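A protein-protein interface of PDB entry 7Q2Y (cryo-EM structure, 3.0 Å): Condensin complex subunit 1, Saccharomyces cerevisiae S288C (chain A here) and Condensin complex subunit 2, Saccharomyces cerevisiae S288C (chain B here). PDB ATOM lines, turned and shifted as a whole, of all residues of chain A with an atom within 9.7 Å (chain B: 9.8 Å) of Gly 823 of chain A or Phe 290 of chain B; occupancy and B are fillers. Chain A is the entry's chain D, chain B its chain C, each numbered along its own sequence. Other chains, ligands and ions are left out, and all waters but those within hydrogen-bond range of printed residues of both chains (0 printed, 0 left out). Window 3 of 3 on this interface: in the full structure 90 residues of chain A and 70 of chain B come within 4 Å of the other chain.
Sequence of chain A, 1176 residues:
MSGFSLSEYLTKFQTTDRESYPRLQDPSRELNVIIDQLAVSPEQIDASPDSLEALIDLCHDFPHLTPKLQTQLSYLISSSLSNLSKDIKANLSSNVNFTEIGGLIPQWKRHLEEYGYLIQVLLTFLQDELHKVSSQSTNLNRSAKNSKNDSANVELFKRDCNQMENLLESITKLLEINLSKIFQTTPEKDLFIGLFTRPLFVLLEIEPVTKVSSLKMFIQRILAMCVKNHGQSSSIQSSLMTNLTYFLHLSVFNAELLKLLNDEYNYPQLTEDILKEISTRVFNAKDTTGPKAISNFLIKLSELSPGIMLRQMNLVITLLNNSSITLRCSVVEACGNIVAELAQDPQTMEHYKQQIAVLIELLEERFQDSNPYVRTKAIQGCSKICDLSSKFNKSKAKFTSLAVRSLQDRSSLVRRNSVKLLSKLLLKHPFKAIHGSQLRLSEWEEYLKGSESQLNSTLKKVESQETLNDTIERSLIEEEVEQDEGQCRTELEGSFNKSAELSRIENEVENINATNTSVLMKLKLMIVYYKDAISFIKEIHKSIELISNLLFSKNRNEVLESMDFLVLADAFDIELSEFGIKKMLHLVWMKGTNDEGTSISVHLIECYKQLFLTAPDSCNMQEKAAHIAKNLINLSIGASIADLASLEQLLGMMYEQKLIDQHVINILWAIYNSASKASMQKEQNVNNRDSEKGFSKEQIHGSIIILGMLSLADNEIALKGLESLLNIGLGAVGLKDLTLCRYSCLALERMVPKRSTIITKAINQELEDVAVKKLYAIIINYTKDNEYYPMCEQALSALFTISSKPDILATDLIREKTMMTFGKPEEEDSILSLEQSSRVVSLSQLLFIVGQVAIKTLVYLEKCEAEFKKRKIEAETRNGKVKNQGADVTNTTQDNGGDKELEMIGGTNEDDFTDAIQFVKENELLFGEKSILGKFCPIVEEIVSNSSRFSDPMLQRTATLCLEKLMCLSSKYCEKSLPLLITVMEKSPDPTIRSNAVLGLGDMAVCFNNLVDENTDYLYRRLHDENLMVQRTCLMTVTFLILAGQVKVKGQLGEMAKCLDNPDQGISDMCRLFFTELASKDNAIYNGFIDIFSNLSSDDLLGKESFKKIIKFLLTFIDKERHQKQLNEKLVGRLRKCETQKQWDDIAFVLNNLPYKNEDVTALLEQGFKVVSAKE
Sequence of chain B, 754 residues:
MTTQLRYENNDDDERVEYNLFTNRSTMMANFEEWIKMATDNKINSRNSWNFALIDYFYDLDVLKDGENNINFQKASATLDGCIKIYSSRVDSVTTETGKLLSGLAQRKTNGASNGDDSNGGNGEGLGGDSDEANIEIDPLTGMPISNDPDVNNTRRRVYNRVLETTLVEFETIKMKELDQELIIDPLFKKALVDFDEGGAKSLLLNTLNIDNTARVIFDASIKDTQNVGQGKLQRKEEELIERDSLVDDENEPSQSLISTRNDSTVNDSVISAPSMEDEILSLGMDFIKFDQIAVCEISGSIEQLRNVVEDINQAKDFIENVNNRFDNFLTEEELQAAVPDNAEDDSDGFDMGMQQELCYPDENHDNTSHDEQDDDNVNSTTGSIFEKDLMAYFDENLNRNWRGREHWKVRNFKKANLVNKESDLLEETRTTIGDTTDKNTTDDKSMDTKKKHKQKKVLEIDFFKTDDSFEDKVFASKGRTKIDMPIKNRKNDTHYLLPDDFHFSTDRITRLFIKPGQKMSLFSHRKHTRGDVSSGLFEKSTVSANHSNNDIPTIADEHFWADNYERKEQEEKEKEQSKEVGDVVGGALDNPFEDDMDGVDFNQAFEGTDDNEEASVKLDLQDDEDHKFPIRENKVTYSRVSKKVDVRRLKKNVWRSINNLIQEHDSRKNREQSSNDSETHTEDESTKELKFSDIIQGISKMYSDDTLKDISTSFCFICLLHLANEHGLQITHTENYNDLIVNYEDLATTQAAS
O of Ile 293 of chain B lies within hydrogen-bond range of NE of Arg 815 of chain A, at 2.9 Å.
The backbone carbonyl oxygen (O) of Ala 294 of chain B lies within hydrogen-bond range of the guanidinium group (NH1) of Arg 815 of chain A (2.7 Å).
The backbone carbonyl oxygen (O) of Cys 296 of chain B lies within hydrogen-bond range of the guanidinium group (NH2) of Arg 815 of chain A (2.4 Å).
The side-chain sulfur of Cys 296 of chain B lies within hydrogen-bond range of the side-chain amino group of Lys 935 of chain A, at 3.3 Å.
O of Gln 292 of chain B is in hydrogen-bond range of SG of Cys 296 of chain B.
SG of Cys 296 of chain B lies within hydrogen-bond range of O of Ile 293 of chain B, 3.3 Å away.
The backbone carbonyl oxygen of Gly 823 of chain A sits at hydrogen-bond distance from the guanidinium group of Arg 839 of chain A (3.2 Å).
Among the printed residues, merely in contact across the chains: Phe 822 of chain A with Ile 280 of chain B, Arg 839 of chain A with Ile 280 of chain B, Arg 815 of chain A with Val 295 of chain B, Ile 932 of chain A with Cys 296 of chain B, Arg 839 of chain A with Leu 281 of chain B, Phe 822 of chain A with Gly 284 of chain B, Lys 935 of chain A with Ile 293 of chain B, Lys 935 of chain A with Gln 292 of chain B, Phe 822 of chain A with Phe 290 of chain B and Gly 823 of chain A with Phe 290 of chain B.
Of the printed residues of chain B, Gly 823 of chain A touches Phe 290 (3.97 Å).
Of chain A, only Phe 822 (3.96 Å) and Gly 823 (3.97 Å) come within 4 Å of Phe 290 of chain B.
No residue of chain A comes within 4 Å of Asp 291 of chain B.
Of the printed residues of chain B, Arg 815 of chain A touches Ile 293 (2.9 Å), Ala 294 (2.7 Å), Val 295 (3.6 Å) and Cys 296 (2.4 Å).
Of the printed residues of chain A, Gln 292 of chain B touches Lys 935.
Of the printed residues of chain A, Cys 296 of chain B touches Arg 815, Ile 932 and Lys 935.
Phe 287 of chain B touches none of the printed residues of chain A.
Ser 837 of chain A touches none of the printed residues of chain B.
The nearest printed residue of chain A that does not touch Phe 290 of chain B is Lys 824 of chain A (5.1 Å).
Hydrophobic or aromatic side chains of chain A that line the printed part of chain B: Phe 822 and Ile 932.
Among the printed residues, 14 pairs touch across the chains.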
ATOM      1  N   ARG A 815     -14.817   7.111  16.528  1.00  0.00           N
ATOM      2  CA  ARG A 815     -15.995   6.268  16.719  1.00  0.00           C
ATOM      3  C   ARG A 815     -15.926   5.028  15.838  1.00  0.00           C
ATOM      4  O   ARG A 815     -16.169   3.905  16.299  1.00  0.00           O
ATOM      5  CB  ARG A 815     -17.265   7.064  16.416  1.00  0.00           C
ATOM      6  CG  ARG A 815     -17.567   8.186  17.390  1.00  0.00           C
ATOM      7  CD  ARG A 815     -18.840   8.909  16.988  1.00  0.00           C
ATOM      8  NE  ARG A 815     -19.159  10.012  17.885  1.00  0.00           N
ATOM      9  CZ  ARG A 815     -20.186  10.835  17.721  1.00  0.00           C
ATOM     10  NH1 ARG A 815     -21.015  10.709  16.698  1.00  0.00           N
ATOM     11  NH2 ARG A 815     -20.385  11.807  18.604  1.00  0.00           N
ATOM     12  N   GLU A 816     -15.587   5.212  14.561  1.00  0.00           N
ATOM     13  CA  GLU A 816     -15.497   4.062  13.668  1.00  0.00           C
ATOM     14  C   GLU A 816     -14.412   3.095  14.125  1.00  0.00           C
ATOM     15  O   GLU A 816     -14.612   1.875  14.095  1.00  0.00           O
ATOM     16  CB  GLU A 816     -15.245   4.506  12.229  1.00  0.00           C
ATOM     17  CG  GLU A 816     -15.829   3.540  11.207  1.00  0.00           C
ATOM     18  CD  GLU A 816     -15.358   3.814   9.795  1.00  0.00           C
ATOM     19  OE1 GLU A 816     -15.022   4.976   9.495  1.00  0.00           O
ATOM     20  OE2 GLU A 816     -15.324   2.864   8.984  1.00  0.00           O
ATOM     21  N   LYS A 817     -13.262   3.616  14.559  1.00  0.00           N
ATOM     22  CA  LYS A 817     -12.174   2.742  14.984  1.00  0.00           C
ATOM     23  C   LYS A 817     -12.529   1.977  16.256  1.00  0.00           C
ATOM     24  O   LYS A 817     -12.226   0.783  16.369  1.00  0.00           O
ATOM     25  CB  LYS A 817     -10.895   3.557  15.182  1.00  0.00           C
ATOM     26  CG  LYS A 817      -9.663   2.716  15.470  1.00  0.00           C
ATOM     27  CD  LYS A 817      -9.448   1.652  14.406  1.00  0.00           C
ATOM     28  CE  LYS A 817      -8.998   2.266  13.092  1.00  0.00           C
ATOM     29  NZ  LYS A 817      -8.763   1.231  12.049  1.00  0.00           N
ATOM     30  N   THR A 818     -13.163   2.645  17.226  1.00  0.00           N
ATOM     31  CA  THR A 818     -13.529   2.003  18.481  1.00  0.00           C
ATOM     32  C   THR A 818     -14.765   1.128  18.354  1.00  0.00           C
ATOM     33  O   THR A 818     -15.112   0.432  19.314  1.00  0.00           O
ATOM     34  CB  THR A 818     -13.757   3.050  19.575  1.00  0.00           C
ATOM     35  OG1 THR A 818     -13.772   2.408  20.856  1.00  0.00           O
ATOM     36  CG2 THR A 818     -15.085   3.762  19.367  1.00  0.00           C
ATOM     37  N   MET A 819     -15.469   1.194  17.224  1.00  0.00           N
ATOM     38  CA  MET A 819     -16.407   0.123  16.904  1.00  0.00           C
ATOM     39  C   MET A 819     -15.692  -1.057  16.249  1.00  0.00           C
ATOM     40  O   MET A 819     -15.862  -2.209  16.676  1.00  0.00           O
ATOM     41  CB  MET A 819     -17.530   0.639  15.999  1.00  0.00           C
ATOM     42  CG  MET A 819     -18.349   1.771  16.594  1.00  0.00           C
ATOM     43  SD  MET A 819     -19.963   1.942  15.810  1.00  0.00           S
ATOM     44  CE  MET A 819     -19.970   3.691  15.427  1.00  0.00           C
ATOM     45  N   MET A 820     -14.883  -0.786  15.216  1.00  0.00           N
ATOM     46  CA  MET A 820     -14.210  -1.859  14.485  1.00  0.00           C
ATOM     47  C   MET A 820     -13.392  -2.736  15.420  1.00  0.00           C
ATOM     48  O   MET A 820     -13.467  -3.968  15.348  1.00  0.00           O
ATOM     49  CB  MET A 820     -13.322  -1.279  13.384  1.00  0.00           C
ATOM     50  CG  MET A 820     -14.084  -0.596  12.265  1.00  0.00           C
ATOM     51  SD  MET A 820     -12.985   0.138  11.043  1.00  0.00           S
ATOM     52  CE  MET A 820     -12.322  -1.329  10.259  1.00  0.00           C
ATOM     53  N   THR A 821     -12.607  -2.130  16.301  1.00  0.00           N
ATOM     54  CA  THR A 821     -12.130  -2.854  17.465  1.00  0.00           C
ATOM     55  C   THR A 821     -13.208  -2.778  18.536  1.00  0.00           C
ATOM     56  O   THR A 821     -13.960  -1.805  18.610  1.00  0.00           O
ATOM     57  CB  THR A 821     -10.800  -2.291  17.980  1.00  0.00           C
ATOM     58  OG1 THR A 821     -10.190  -3.239  18.865  1.00  0.00           O
ATOM     59  CG2 THR A 821     -11.006  -0.980  18.722  1.00  0.00           C
ATOM     60  N   PHE A 822     -13.316  -3.841  19.327  1.00  0.00           N
ATOM     61  CA  PHE A 822     -14.293  -4.031  20.398  1.00  0.00           C
ATOM     62  C   PHE A 822     -15.686  -4.396  19.883  1.00  0.00           C
ATOM     63  O   PHE A 822     -16.584  -4.586  20.715  1.00  0.00           O
ATOM     64  CB  PHE A 822     -14.425  -2.813  21.329  1.00  0.00           C
ATOM     65  CG  PHE A 822     -13.154  -2.453  22.044  1.00  0.00           C
ATOM     66  CD1 PHE A 822     -12.405  -3.424  22.685  1.00  0.00           C
ATOM     67  CD2 PHE A 822     -12.712  -1.142  22.076  1.00  0.00           C
ATOM     68  CE1 PHE A 822     -11.235  -3.093  23.344  1.00  0.00           C
ATOM     69  CE2 PHE A 822     -11.545  -0.805  22.732  1.00  0.00           C
ATOM     70  CZ  PHE A 822     -10.806  -1.781  23.367  1.00  0.00           C
ATOM     71  N   GLY A 823     -15.917  -4.505  18.569  1.00  0.00           N
ATOM     72  CA  GLY A 823     -17.106  -5.203  18.125  1.00  0.00           C
ATOM     73  C   GLY A 823     -16.864  -5.901  16.805  1.00  0.00           C
ATOM     74  O   GLY A 823     -15.810  -5.756  16.181  1.00  0.00           O
ATOM     75  N   LYS A 824     -17.865  -6.667  16.386  1.00  0.00           N
ATOM     76  CA  LYS A 824     -17.786  -7.417  15.138  1.00  0.00           C
ATOM     77  C   LYS A 824     -18.736  -6.843  14.092  1.00  0.00           C
ATOM     78  O   LYS A 824     -18.569  -5.708  13.645  1.00  0.00           O
ATOM     79  CB  LYS A 824     -18.101  -8.895  15.380  1.00  0.00           C
ATOM     80  CG  LYS A 824     -17.107  -9.598  16.289  1.00  0.00           C
ATOM     81  CD  LYS A 824     -17.545 -11.022  16.593  1.00  0.00           C
ATOM     82  CE  LYS A 824     -16.562 -11.714  17.524  1.00  0.00           C
ATOM     83  NZ  LYS A 824     -16.997 -13.095  17.868  1.00  0.00           N
ATOM     84  N   SER A 837      -7.908  -7.587  11.708  1.00  0.00           N
ATOM     85  CA  SER A 837      -7.727  -9.000  12.017  1.00  0.00           C
ATOM     86  C   SER A 837      -7.265  -9.188  13.459  1.00  0.00           C
ATOM     87  O   SER A 837      -7.875  -9.939  14.221  1.00  0.00           O
ATOM     88  CB  SER A 837      -6.722  -9.637  11.055  1.00  0.00           C
ATOM     89  OG  SER A 837      -5.441  -9.048  11.190  1.00  0.00           O
ATOM     90  N   ARG A 839      -6.954  -7.803  17.048  1.00  0.00           N
ATOM     91  CA  ARG A 839      -7.522  -6.794  17.933  1.00  0.00           C
ATOM     92  C   ARG A 839      -6.438  -6.018  18.664  1.00  0.00           C
ATOM     93  O   ARG A 839      -6.630  -4.840  18.976  1.00  0.00           O
ATOM     94  CB  ARG A 839      -8.476  -7.448  18.931  1.00  0.00           C
ATOM     95  CG  ARG A 839      -9.577  -8.268  18.285  1.00  0.00           C
ATOM     96  CD  ARG A 839     -10.929  -7.940  18.889  1.00  0.00           C
ATOM     97  NE  ARG A 839     -12.017  -8.615  18.191  1.00  0.00           N
ATOM     98  CZ  ARG A 839     -13.015  -7.992  17.579  1.00  0.00           C
ATOM     99  NH1 ARG A 839     -13.097  -6.672  17.562  1.00  0.00           N
ATOM    100  NH2 ARG A 839     -13.953  -8.711  16.972  1.00  0.00           N
ATOM    101  N   SER A 842      -5.342  -3.423  16.272  1.00  0.00           N
ATOM    102  CA  SER A 842      -6.433  -2.461  16.144  1.00  0.00           C
ATOM    103  C   SER A 842      -6.473  -1.505  17.332  1.00  0.00           C
ATOM    104  O   SER A 842      -6.620  -0.290  17.160  1.00  0.00           O
ATOM    105  CB  SER A 842      -7.765  -3.197  16.002  1.00  0.00           C
ATOM    106  OG  SER A 842      -7.764  -4.040  14.864  1.00  0.00           O
ATOM    107  N   LEU A 846      -5.863   2.507  17.440  1.00  0.00           N
ATOM    108  CA  LEU A 846      -6.860   3.391  18.036  1.00  0.00           C
ATOM    109  C   LEU A 846      -6.239   4.301  19.090  1.00  0.00           C
ATOM    110  O   LEU A 846      -6.543   5.497  19.143  1.00  0.00           O
ATOM    111  CB  LEU A 846      -7.994   2.563  18.640  1.00  0.00           C
ATOM    112  CG  LEU A 846      -9.024   3.292  19.503  1.00  0.00           C
ATOM    113  CD1 LEU A 846      -9.691   4.418  18.727  1.00  0.00           C
ATOM    114  CD2 LEU A 846     -10.060   2.310  20.023  1.00  0.00           C
ATOM    115  N   ILE A 932     -15.339  11.823  24.315  1.00  0.00           N
ATOM    116  CA  ILE A 932     -14.936  10.474  23.934  1.00  0.00           C
ATOM    117  C   ILE A 932     -13.481  10.245  24.329  1.00  0.00           C
ATOM    118  O   ILE A 932     -13.055   9.104  24.535  1.00  0.00           O
ATOM    119  CB  ILE A 932     -15.157  10.232  22.428  1.00  0.00           C
ATOM    120  CG1 ILE A 932     -14.980   8.751  22.086  1.00  0.00           C
ATOM    121  CG2 ILE A 932     -14.215  11.083  21.599  1.00  0.00           C
ATOM    122  CD1 ILE A 932     -15.489   8.380  20.711  1.00  0.00           C
ATOM    123  N   LYS A 935     -13.025   8.727  28.200  1.00  0.00           N
ATOM    124  CA  LYS A 935     -13.237   7.312  28.477  1.00  0.00           C
ATOM    125  C   LYS A 935     -12.084   6.433  28.009  1.00  0.00           C
ATOM    126  O   LYS A 935     -12.045   5.252  28.372  1.00  0.00           O
ATOM    127  CB  LYS A 935     -14.545   6.836  27.839  1.00  0.00           C
ATOM    128  CG  LYS A 935     -14.597   6.970  26.331  1.00  0.00           C
ATOM    129  CD  LYS A 935     -15.876   6.365  25.777  1.00  0.00           C
ATOM    130  CE  LYS A 935     -17.096   7.168  26.199  1.00  0.00           C
ATOM    131  NZ  LYS A 935     -17.107   8.531  25.603  1.00  0.00           N
ATOM    132  N   GLU B 277      -7.263 -11.969  22.551  1.00  0.00           N
ATOM    133  CA  GLU B 277      -8.521 -11.400  22.080  1.00  0.00           C
ATOM    134  C   GLU B 277      -9.595 -11.475  23.159  1.00  0.00           C
ATOM    135  O   GLU B 277     -10.427 -10.570  23.277  1.00  0.00           O
ATOM    136  CB  GLU B 277      -8.969 -12.100  20.792  1.00  0.00           C
ATOM    137  CG  GLU B 277      -9.862 -13.322  20.974  1.00  0.00           C
ATOM    138  CD  GLU B 277      -9.099 -14.555  21.427  1.00  0.00           C
ATOM    139  OE1 GLU B 277      -7.866 -14.468  21.607  1.00  0.00           O
ATOM    140  OE2 GLU B 277      -9.737 -15.614  21.602  1.00  0.00           O
ATOM    141  N   ILE B 280      -8.934  -8.595  25.404  1.00  0.00           N
ATOM    142  CA  ILE B 280      -9.324  -7.336  24.774  1.00  0.00           C
ATOM    143  C   ILE B 280     -10.837  -7.156  24.812  1.00  0.00           C
ATOM    144  O   ILE B 280     -11.334  -6.063  25.106  1.00  0.00           O
ATOM    145  CB  ILE B 280      -8.776  -7.266  23.339  1.00  0.00           C
ATOM    146  CG1 ILE B 280      -7.249  -7.197  23.370  1.00  0.00           C
ATOM    147  CG2 ILE B 280      -9.357  -6.069  22.599  1.00  0.00           C
ATOM    148  CD1 ILE B 280      -6.637  -6.760  22.072  1.00  0.00           C
ATOM    149  N   LEU B 281     -11.593  -8.216  24.511  1.00  0.00           N
ATOM    150  CA  LEU B 281     -13.048  -8.127  24.602  1.00  0.00           C
ATOM    151  C   LEU B 281     -13.506  -7.876  26.034  1.00  0.00           C
ATOM    152  O   LEU B 281     -14.454  -7.117  26.262  1.00  0.00           O
ATOM    153  CB  LEU B 281     -13.705  -9.390  24.040  1.00  0.00           C
ATOM    154  CG  LEU B 281     -13.980  -9.473  22.532  1.00  0.00           C
ATOM    155  CD1 LEU B 281     -14.992  -8.408  22.134  1.00  0.00           C
ATOM    156  CD2 LEU B 281     -12.727  -9.339  21.690  1.00  0.00           C
ATOM    157  N   GLY B 284     -12.859  -4.233  26.738  1.00  0.00           N
ATOM    158  CA  GLY B 284     -13.842  -3.422  26.039  1.00  0.00           C
ATOM    159  C   GLY B 284     -15.194  -3.440  26.723  1.00  0.00           C
ATOM    160  O   GLY B 284     -15.815  -2.397  26.923  1.00  0.00           O
ATOM    161  N   MET B 285     -15.659  -4.631  27.108  1.00  0.00           N
ATOM    162  CA  MET B 285     -16.929  -4.734  27.820  1.00  0.00           C
ATOM    163  C   MET B 285     -16.876  -3.985  29.145  1.00  0.00           C
ATOM    164  O   MET B 285     -17.871  -3.385  29.569  1.00  0.00           O
ATOM    165  CB  MET B 285     -17.286  -6.204  28.046  1.00  0.00           C
ATOM    166  CG  MET B 285     -18.139  -6.812  26.945  1.00  0.00           C
ATOM    167  SD  MET B 285     -19.813  -6.143  26.914  1.00  0.00           S
ATOM    168  CE  MET B 285     -20.492  -6.860  28.408  1.00  0.00           C
ATOM    169  N   ASP B 286     -15.723  -4.014  29.816  1.00  0.00           N
ATOM    170  CA  ASP B 286     -15.584  -3.294  31.077  1.00  0.00           C
ATOM    171  C   ASP B 286     -15.642  -1.785  30.873  1.00  0.00           C
ATOM    172  O   ASP B 286     -16.241  -1.069  31.684  1.00  0.00           O
ATOM    173  CB  ASP B 286     -14.278  -3.691  31.764  1.00  0.00           C
ATOM    174  CG  ASP B 286     -14.451  -4.854  32.721  1.00  0.00           C
ATOM    175  OD1 ASP B 286     -15.459  -5.581  32.597  1.00  0.00           O
ATOM    176  OD2 ASP B 286     -13.581  -5.040  33.596  1.00  0.00           O
ATOM    177  N   PHE B 287     -15.029  -1.277  29.800  1.00  0.00           N
ATOM    178  CA  PHE B 287     -14.856   0.160  29.635  1.00  0.00           C
ATOM    179  C   PHE B 287     -15.605   0.777  28.460  1.00  0.00           C
ATOM    180  O   PHE B 287     -15.844   1.989  28.483  1.00  0.00           O
ATOM    181  CB  PHE B 287     -13.365   0.506  29.493  1.00  0.00           C
ATOM    182  CG  PHE B 287     -12.531   0.087  30.670  1.00  0.00           C
ATOM    183  CD1 PHE B 287     -12.760   0.627  31.924  1.00  0.00           C
ATOM    184  CD2 PHE B 287     -11.517  -0.843  30.522  1.00  0.00           C
ATOM    185  CE1 PHE B 287     -11.996   0.245  33.010  1.00  0.00           C
ATOM    186  CE2 PHE B 287     -10.748  -1.230  31.604  1.00  0.00           C
ATOM    187  CZ  PHE B 287     -10.988  -0.684  32.849  1.00  0.00           C
ATOM    188  N   ILE B 288     -15.980   0.003  27.445  1.00  0.00           N
ATOM    189  CA  ILE B 288     -16.596   0.537  26.235  1.00  0.00           C
ATOM    190  C   ILE B 288     -17.976  -0.080  26.059  1.00  0.00           C
ATOM    191  O   ILE B 288     -18.126  -1.306  26.102  1.00  0.00           O
ATOM    192  CB  ILE B 288     -15.724   0.284  24.992  1.00  0.00           C
ATOM    193  CG1 ILE B 288     -14.351   0.932  25.167  1.00  0.00           C
ATOM    194  CG2 ILE B 288     -16.408   0.809  23.739  1.00  0.00           C
ATOM    195  CD1 ILE B 288     -14.418   2.434  25.337  1.00  0.00           C
ATOM    196  N   LYS B 289     -18.974   0.771  25.853  1.00  0.00           N
ATOM    197  CA  LYS B 289     -20.329   0.348  25.536  1.00  0.00           C
ATOM    198  C   LYS B 289     -20.710   0.903  24.172  1.00  0.00           C
ATOM    199  O   LYS B 289     -20.261   1.987  23.789  1.00  0.00           O
ATOM    200  CB  LYS B 289     -21.322   0.820  26.601  1.00  0.00           C
ATOM    201  CG  LYS B 289     -21.008   0.328  28.004  1.00  0.00           C
ATOM    202  CD  LYS B 289     -21.540   1.286  29.058  1.00  0.00           C
ATOM    203  CE  LYS B 289     -21.786   0.573  30.377  1.00  0.00           C
ATOM    204  NZ  LYS B 289     -22.769  -0.535  30.234  1.00  0.00           N
ATOM    205  N   PHE B 290     -21.529   0.149  23.433  1.00  0.00           N
ATOM    206  CA  PHE B 290     -21.921   0.582  22.096  1.00  0.00           C
ATOM    207  C   PHE B 290     -22.682   1.901  22.142  1.00  0.00           C
ATOM    208  O   PHE B 290     -22.449   2.790  21.314  1.00  0.00           O
ATOM    209  CB  PHE B 290     -22.752  -0.503  21.413  1.00  0.00           C
ATOM    210  CG  PHE B 290     -21.929  -1.604  20.807  1.00  0.00           C
ATOM    211  CD1 PHE B 290     -20.580  -1.416  20.548  1.00  0.00           C
ATOM    212  CD2 PHE B 290     -22.502  -2.826  20.495  1.00  0.00           C
ATOM    213  CE1 PHE B 290     -19.818  -2.425  19.991  1.00  0.00           C
ATOM    214  CE2 PHE B 290     -21.744  -3.841  19.937  1.00  0.00           C
ATOM    215  CZ  PHE B 290     -20.402  -3.639  19.685  1.00  0.00           C
ATOM    216  N   ASP B 291     -23.595   2.046  23.097  1.00  0.00           N
ATOM    217  CA  ASP B 291     -24.253   3.326  23.299  1.00  0.00           C
ATOM    218  C   ASP B 291     -23.293   4.313  23.957  1.00  0.00           C
ATOM    219  O   ASP B 291     -22.219   3.946  24.445  1.00  0.00           O
ATOM    220  CB  ASP B 291     -25.514   3.158  24.148  1.00  0.00           C
ATOM    221  CG  ASP B 291     -25.275   2.325  25.390  1.00  0.00           C
ATOM    222  OD1 ASP B 291     -24.169   1.765  25.527  1.00  0.00           O
ATOM    223  OD2 ASP B 291     -26.196   2.227  26.229  1.00  0.00           O
ATOM    224  N   GLN B 292     -23.690   5.587  23.952  1.00  0.00           N
ATOM    225  CA  GLN B 292     -22.898   6.694  24.479  1.00  0.00           C
ATOM    226  C   GLN B 292     -21.580   6.879  23.736  1.00  0.00           C
ATOM    227  O   GLN B 292     -20.647   7.487  24.270  1.00  0.00           O
ATOM    228  CB  GLN B 292     -22.634   6.534  25.982  1.00  0.00           C
ATOM    229  CG  GLN B 292     -23.883   6.612  26.844  1.00  0.00           C
ATOM    230  CD  GLN B 292     -23.789   5.747  28.085  1.00  0.00           C
ATOM    231  OE1 GLN B 292     -22.779   5.757  28.788  1.00  0.00           O
ATOM    232  NE2 GLN B 292     -24.846   4.992  28.362  1.00  0.00           N
ATOM    233  N   ILE B 293     -21.481   6.362  22.513  1.00  0.00           N
ATOM    234  CA  ILE B 293     -20.318   6.562  21.664  1.00  0.00           C
ATOM    235  C   ILE B 293     -20.647   7.439  20.463  1.00  0.00           C
ATOM    236  O   ILE B 293     -19.880   8.343  20.122  1.00  0.00           O
ATOM    237  CB  ILE B 293     -19.729   5.206  21.213  1.00  0.00           C
ATOM    238  CG1 ILE B 293     -18.981   4.539  22.367  1.00  0.00           C
ATOM    239  CG2 ILE B 293     -18.807   5.385  20.016  1.00  0.00           C
ATOM    240  CD1 ILE B 293     -17.753   5.298  22.816  1.00  0.00           C
ATOM    241  N   ALA B 294     -21.789   7.201  19.822  1.00  0.00           N
ATOM    242  CA  ALA B 294     -22.223   8.003  18.687  1.00  0.00           C
ATOM    243  C   ALA B 294     -22.821   9.340  19.102  1.00  0.00           C
ATOM    244  O   ALA B 294     -23.135  10.157  18.228  1.00  0.00           O
ATOM    245  CB  ALA B 294     -23.238   7.222  17.848  1.00  0.00           C
ATOM    246  N   VAL B 295     -22.991   9.583  20.399  1.00  0.00           N
ATOM    247  CA  VAL B 295     -23.521  10.850  20.881  1.00  0.00           C
ATOM    248  C   VAL B 295     -22.459  11.724  21.536  1.00  0.00           C
ATOM    249  O   VAL B 295     -22.679  12.939  21.666  1.00  0.00           O
ATOM    250  CB  VAL B 295     -24.701  10.630  21.851  1.00  0.00           C
ATOM    251  CG1 VAL B 295     -25.820   9.866  21.161  1.00  0.00           C
ATOM    252  CG2 VAL B 295     -24.233   9.895  23.097  1.00  0.00           C
ATOM    253  N   CYS B 296     -21.327  11.160  21.949  1.00  0.00           N
ATOM    254  CA  CYS B 296     -20.258  11.930  22.571  1.00  0.00           C
ATOM    255  C   CYS B 296     -19.322  12.474  21.498  1.00  0.00           C
ATOM    256  O   CYS B 296     -18.977  11.765  20.547  1.00  0.00           O
ATOM    257  CB  CYS B 296     -19.486  11.072  23.573  1.00  0.00           C
ATOM    258  SG  CYS B 296     -18.672   9.625  22.860  1.00  0.00           S
